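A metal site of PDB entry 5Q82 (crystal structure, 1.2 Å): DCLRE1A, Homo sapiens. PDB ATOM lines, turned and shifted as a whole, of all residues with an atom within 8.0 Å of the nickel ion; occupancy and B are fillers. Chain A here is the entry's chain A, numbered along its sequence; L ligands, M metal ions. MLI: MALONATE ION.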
ATOM      1  N   ASP A  18      -2.038  21.027  11.989  1.00  0.00           N
ATOM      2  CA  ASP A  18      -1.340  20.426  13.170  1.00  0.00           C
ATOM      3  C   ASP A  18      -1.931  20.957  14.555  1.00  0.00           C
ATOM      4  O   ASP A  18      -1.165  21.258  15.506  1.00  0.00           O
ATOM      5  CB  ASP A  18       0.174  20.580  13.057  1.00  0.00           C
ATOM      6  CG  ASP A  18       0.736  19.897  11.763  1.00  0.00           C
ATOM      7  OD1 ASP A  18       0.022  19.128  11.124  1.00  0.00           O
ATOM      8  OD2 ASP A  18       1.971  20.193  11.519  1.00  0.00           O
ATOM      9  N   THR A  34       0.326  17.538   8.828  1.00  0.00           N
ATOM     10  CA  THR A  34       1.465  17.562   7.915  1.00  0.00           C
ATOM     11  C   THR A  34       2.296  16.247   7.941  1.00  0.00           C
ATOM     12  O   THR A  34       2.824  15.817   6.898  1.00  0.00           O
ATOM     13  CB  THR A  34       2.398  18.758   8.078  1.00  0.00           C
ATOM     14  OG1 THR A  34       2.973  18.701   9.436  1.00  0.00           O
ATOM     15  CG2 THR A  34       1.663  20.118   7.886  1.00  0.00           C
ATOM     16  N   HIS A  35       2.380  15.625   9.136  1.00  0.00           N
ATOM     17  CA  HIS A  35       3.201  14.414   9.318  1.00  0.00           C
ATOM     18  C   HIS A  35       2.907  13.796  10.665  1.00  0.00           C
ATOM     19  O   HIS A  35       2.451  14.480  11.627  1.00  0.00           O
ATOM     20  CB  HIS A  35       4.750  14.738   9.111  1.00  0.00           C
ATOM     21  CG  HIS A  35       5.391  15.606  10.132  1.00  0.00           C
ATOM     22  ND1 HIS A  35       5.130  16.942  10.341  1.00  0.00           N
ATOM     23  CD2 HIS A  35       6.378  15.307  11.013  1.00  0.00           C
ATOM     24  CE1 HIS A  35       5.942  17.388  11.306  1.00  0.00           C
ATOM     25  NE2 HIS A  35       6.712  16.423  11.706  1.00  0.00           N
ATOM     26  N   PHE A  36       3.329  12.517  10.741  1.00  0.00           N
ATOM     27  CA  PHE A  36       3.114  11.695  11.950  1.00  0.00           C
ATOM     28  C   PHE A  36       4.275  11.826  12.953  1.00  0.00           C
ATOM     29  O   PHE A  36       5.006  10.786  13.215  1.00  0.00           O
ATOM     30  CB  PHE A  36       2.881  10.228  11.527  1.00  0.00           C
ATOM     31  CG  PHE A  36       2.250   9.362  12.602  1.00  0.00           C
ATOM     32  CD1 PHE A  36       0.875   9.487  12.907  1.00  0.00           C
ATOM     33  CD2 PHE A  36       3.019   8.439  13.313  1.00  0.00           C
ATOM     34  CE1 PHE A  36       0.281   8.686  13.916  1.00  0.00           C
ATOM     35  CE2 PHE A  36       2.419   7.606  14.296  1.00  0.00           C
ATOM     36  CZ  PHE A  36       1.092   7.722  14.570  1.00  0.00           C
ATOM     37  N   HIS A  37       4.438  13.010  13.596  1.00  0.00           N
ATOM     38  CA  HIS A  37       5.312  13.231  14.763  1.00  0.00           C
ATOM     39  C   HIS A  37       4.413  13.741  15.895  1.00  0.00           C
ATOM     40  O   HIS A  37       3.494  14.525  15.695  1.00  0.00           O
ATOM     41  CB  HIS A  37       6.469  14.204  14.497  1.00  0.00           C
ATOM     42  CG  HIS A  37       7.652  13.611  13.754  1.00  0.00           C
ATOM     43  ND1 HIS A  37       8.633  14.363  13.115  1.00  0.00           N
ATOM     44  CD2 HIS A  37       8.037  12.333  13.607  1.00  0.00           C
ATOM     45  CE1 HIS A  37       9.576  13.565  12.653  1.00  0.00           C
ATOM     46  NE2 HIS A  37       9.225  12.331  12.922  1.00  0.00           N
ATOM     47  N   SER A  38       4.703  13.240  17.125  1.00  0.00           N
ATOM     48  CA  SER A  38       3.799  13.414  18.302  1.00  0.00           C
ATOM     49  C   SER A  38       3.535  14.868  18.614  1.00  0.00           C
ATOM     50  O   SER A  38       2.333  15.137  18.945  1.00  0.00           O
ATOM     51  CB  SER A  38       4.248  12.549  19.474  1.00  0.00           C
ATOM     52  OG  SER A  38       5.512  12.976  19.881  1.00  0.00           O
ATOM     53  N   ASP A  39       4.485  15.771  18.489  1.00  0.00           N
ATOM     54  CA  ASP A  39       4.177  17.220  18.795  1.00  0.00           C
ATOM     55  C   ASP A  39       3.114  17.772  17.818  1.00  0.00           C
ATOM     56  O   ASP A  39       2.435  18.799  18.122  1.00  0.00           O
ATOM     57  CB  ASP A  39       5.407  18.103  18.741  1.00  0.00           C
ATOM     58  CG  ASP A  39       6.324  18.041  20.012  1.00  0.00           C
ATOM     59  OD1 ASP A  39       5.904  17.388  20.995  1.00  0.00           O
ATOM     60  OD2 ASP A  39       7.387  18.666  19.973  1.00  0.00           O
ATOM     61  N   HIS A  40       2.985  17.148  16.616  1.00  0.00           N
ATOM     62  CA  HIS A  40       2.027  17.604  15.601  1.00  0.00           C
ATOM     63  C   HIS A  40       0.716  16.889  15.645  1.00  0.00           C
ATOM     64  O   HIS A  40      -0.352  17.531  15.413  1.00  0.00           O
ATOM     65  CB  HIS A  40       2.736  17.487  14.177  1.00  0.00           C
ATOM     66  CG  HIS A  40       3.936  18.343  14.071  1.00  0.00           C
ATOM     67  ND1 HIS A  40       3.975  19.568  13.444  1.00  0.00           N
ATOM     68  CD2 HIS A  40       5.203  18.169  14.567  1.00  0.00           C
ATOM     69  CE1 HIS A  40       5.150  20.127  13.578  1.00  0.00           C
ATOM     70  NE2 HIS A  40       5.917  19.291  14.285  1.00  0.00           N
ATOM     71  N   HIS A  96      11.193  15.465   4.844  1.00  0.00           N
ATOM     72  CA  HIS A  96      11.273  15.366   6.322  1.00  0.00           C
ATOM     73  C   HIS A  96      11.268  13.877   6.587  1.00  0.00           C
ATOM     74  O   HIS A  96      12.263  13.193   6.167  1.00  0.00           O
ATOM     75  CB  HIS A  96      10.204  16.203   7.023  1.00  0.00           C
ATOM     76  CG  HIS A  96      10.236  16.263   8.528  1.00  0.00           C
ATOM     77  ND1 HIS A  96      11.369  16.598   9.236  1.00  0.00           N
ATOM     78  CD2 HIS A  96       9.270  15.994   9.449  1.00  0.00           C
ATOM     79  CE1 HIS A  96      11.078  16.562  10.539  1.00  0.00           C
ATOM     80  NE2 HIS A  96       9.812  16.229  10.723  1.00  0.00           N
ATOM     81  N   CYS A  97      10.313  13.336   7.288  1.00  0.00           N
ATOM     82  CA  CYS A  97      10.144  11.849   7.516  1.00  0.00           C
ATOM     83  C   CYS A  97       9.153  11.279   6.490  1.00  0.00           C
ATOM     84  O   CYS A  97       8.486  12.024   5.773  1.00  0.00           O
ATOM     85  CB  CYS A  97       9.662  11.675   8.984  1.00  0.00           C
ATOM     86  SG  CYS A  97       7.960  12.371   9.305  1.00  0.00           S
ATOM     87  N   ALA A 100       5.603  13.001   5.185  1.00  0.00           N
ATOM     88  CA  ALA A 100       5.573  14.432   5.570  1.00  0.00           C
ATOM     89  C   ALA A 100       5.356  15.276   4.296  1.00  0.00           C
ATOM     90  O   ALA A 100       6.002  15.104   3.261  1.00  0.00           O
ATOM     91  CB  ALA A 100       6.812  14.845   6.263  1.00  0.00           C
ATOM     92  N   GLY A 117       4.990  22.744   6.947  1.00  0.00           N
ATOM     93  CA  GLY A 117       5.086  21.749   8.000  1.00  0.00           C
ATOM     94  C   GLY A 117       6.491  21.734   8.555  1.00  0.00           C
ATOM     95  O   GLY A 117       7.124  22.771   8.705  1.00  0.00           O
ATOM     96  N   ASP A 118       6.992  20.533   8.928  1.00  0.00           N
ATOM     97  CA  ASP A 118       8.452  20.354   9.129  1.00  0.00           C
ATOM     98  C   ASP A 118       9.113  19.982   7.769  1.00  0.00           C
ATOM     99  O   ASP A 118       8.577  19.138   7.039  1.00  0.00           O
ATOM    100  CB  ASP A 118       8.747  19.263  10.159  1.00  0.00           C
ATOM    101  CG  ASP A 118       8.546  19.660  11.621  1.00  0.00           C
ATOM    102  OD1 ASP A 118       8.395  20.869  11.920  1.00  0.00           O
ATOM    103  OD2 ASP A 118       8.692  18.790  12.497  1.00  0.00           O
ATOM    104  N   PHE A 119      10.263  20.589   7.460  1.00  0.00           N
ATOM    105  CA  PHE A 119      10.896  20.297   6.155  1.00  0.00           C
ATOM    106  C   PHE A 119      12.414  20.446   6.208  1.00  0.00           C
ATOM    107  O   PHE A 119      12.947  21.143   7.065  1.00  0.00           O
ATOM    108  CB  PHE A 119      10.271  21.152   4.986  1.00  0.00           C
ATOM    109  CG  PHE A 119      10.805  22.576   4.716  1.00  0.00           C
ATOM    110  CD1 PHE A 119      10.996  23.056   3.426  1.00  0.00           C
ATOM    111  CD2 PHE A 119      11.106  23.473   5.758  1.00  0.00           C
ATOM    112  CE1 PHE A 119      11.419  24.351   3.170  1.00  0.00           C
ATOM    113  CE2 PHE A 119      11.541  24.774   5.503  1.00  0.00           C
ATOM    114  CZ  PHE A 119      11.700  25.211   4.194  1.00  0.00           C
ATOM    115  N   ASP A 141       9.010  26.390   8.873  1.00  0.00           N
ATOM    116  CA  ASP A 141       9.777  25.609   9.910  1.00  0.00           C
ATOM    117  C   ASP A 141      11.125  26.248  10.069  1.00  0.00           C
ATOM    118  O   ASP A 141      12.058  26.125   9.279  1.00  0.00           O
ATOM    119  CB  ASP A 141       9.956  24.154   9.399  1.00  0.00           C
ATOM    120  CG  ASP A 141      10.949  23.322  10.214  1.00  0.00           C
ATOM    121  OD1 ASP A 141      11.291  23.797  11.343  1.00  0.00           O
ATOM    122  OD2 ASP A 141      11.328  22.246   9.726  1.00  0.00           O
ATOM    123  N   THR A 143      13.179  25.740  12.774  1.00  0.00           N
ATOM    124  CA  THR A 143      13.897  25.010  13.815  1.00  0.00           C
ATOM    125  C   THR A 143      15.332  25.443  13.951  1.00  0.00           C
ATOM    126  O   THR A 143      15.782  25.754  15.125  1.00  0.00           O
ATOM    127  CB  THR A 143      13.805  23.453  13.543  1.00  0.00           C
ATOM    128  OG1 THR A 143      12.453  22.986  13.570  1.00  0.00           O
ATOM    129  CG2 THR A 143      14.603  22.622  14.604  1.00  0.00           C
ATOM    130  N   SER A 183      10.814   7.723  16.924  1.00  0.00           N
ATOM    131  CA  SER A 183       9.774   8.244  16.039  1.00  0.00           C
ATOM    132  C   SER A 183      10.055   7.738  14.629  1.00  0.00           C
ATOM    133  O   SER A 183      11.173   7.188  14.391  1.00  0.00           O
ATOM    134  CB  SER A 183       9.797   9.771  15.996  1.00  0.00           C
ATOM    135  OG  SER A 183      11.072  10.225  15.568  1.00  0.00           O
ATOM    136  N   ILE A 184       9.169   7.908  13.683  1.00  0.00           N
ATOM    137  CA  ILE A 184       9.488   7.691  12.303  1.00  0.00           C
ATOM    138  C   ILE A 184      10.458   8.775  11.834  1.00  0.00           C
ATOM    139  O   ILE A 184      10.628   9.849  12.475  1.00  0.00           O
ATOM    140  CB  ILE A 184       8.247   7.641  11.397  1.00  0.00           C
ATOM    141  CG1 ILE A 184       7.491   8.964  11.289  1.00  0.00           C
ATOM    142  CG2 ILE A 184       7.332   6.475  11.786  1.00  0.00           C
ATOM    143  CD1 ILE A 184       6.473   9.039  10.204  1.00  0.00           C
ATOM    144  N   GLU A 296      16.763  15.909   9.558  1.00  0.00           N
ATOM    145  CA  GLU A 296      15.571  16.028   8.693  1.00  0.00           C
ATOM    146  C   GLU A 296      14.922  17.432   8.713  1.00  0.00           C
ATOM    147  O   GLU A 296      13.755  17.624   8.334  1.00  0.00           O
ATOM    148  CB  GLU A 296      14.591  14.885   8.873  1.00  0.00           C
ATOM    149  CG  GLU A 296      15.153  13.509   8.413  1.00  0.00           C
ATOM    150  CD  GLU A 296      14.202  12.344   8.478  1.00  0.00           C
ATOM    151  OE1 GLU A 296      13.177  12.356   9.220  1.00  0.00           O
ATOM    152  OE2 GLU A 296      14.520  11.300   7.778  1.00  0.00           O
ATOM    153  N   HIS A 297      15.700  18.431   9.222  1.00  0.00           N
ATOM    154  CA  HIS A 297      15.323  19.850   9.110  1.00  0.00           C
ATOM    155  C   HIS A 297      16.395  20.652   8.335  1.00  0.00           C
ATOM    156  O   HIS A 297      17.581  20.294   8.324  1.00  0.00           O
ATOM    157  CB  HIS A 297      15.142  20.523  10.520  1.00  0.00           C
ATOM    158  CG  HIS A 297      14.051  19.972  11.375  1.00  0.00           C
ATOM    159  ND1 HIS A 297      12.744  20.410  11.322  1.00  0.00           N
ATOM    160  CD2 HIS A 297      14.092  19.048  12.397  1.00  0.00           C
ATOM    161  CE1 HIS A 297      12.031  19.785  12.261  1.00  0.00           C
ATOM    162  NE2 HIS A 297      12.825  18.928  12.863  1.00  0.00           N
HETATM  163  C1  MLI L   1      10.051  16.314  15.750  1.00  0.00           C
HETATM  164  C2  MLI L   1      11.072  16.829  14.715  1.00  0.00           C
HETATM  165  C3  MLI L   1       8.681  17.049  15.658  1.00  0.00           C
HETATM  166  O6  MLI L   1      12.216  17.233  14.993  1.00  0.00           O
HETATM  167  O7  MLI L   1      10.722  16.794  13.564  1.00  0.00           O
HETATM  168  O8  MLI L   1       8.065  17.076  14.586  1.00  0.00           O
HETATM  169  O9  MLI L   1       8.161  17.451  16.769  1.00  0.00           O
HETATM  170 NI    NI M   1       8.721  16.598  12.699  1.00  0.00          NI
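The nickel ion is bound by O8 of the ligand, O7 of the ligand, OD2 of Asp 118, NE2 of His 35, ND1 of His 37 and NE2 of His 96.
Four residues have an atom within 4 Å of the nickel ion: His 35, His 37, His 96 and Asp 118. The nearest printed residue that does not touch the nickel ion is His 40 (4.2 Å).
A ring nitrogen (ND1) of His 96 is in hydrogen-bond range of the backbone carbonyl oxygen (O) of Glu 296. A ring nitrogen (NE2) of His 37 is in hydrogen-bond range of the backbone carbonyl oxygen (O) of Ile 184. The side-chain carboxylate of Asp 118 sits close to a ring nitrogen (NE2) of His 40. OG1 of Thr 34 sits at hydrogen-bond distance from ND1 of His 35 (2.9 Å).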
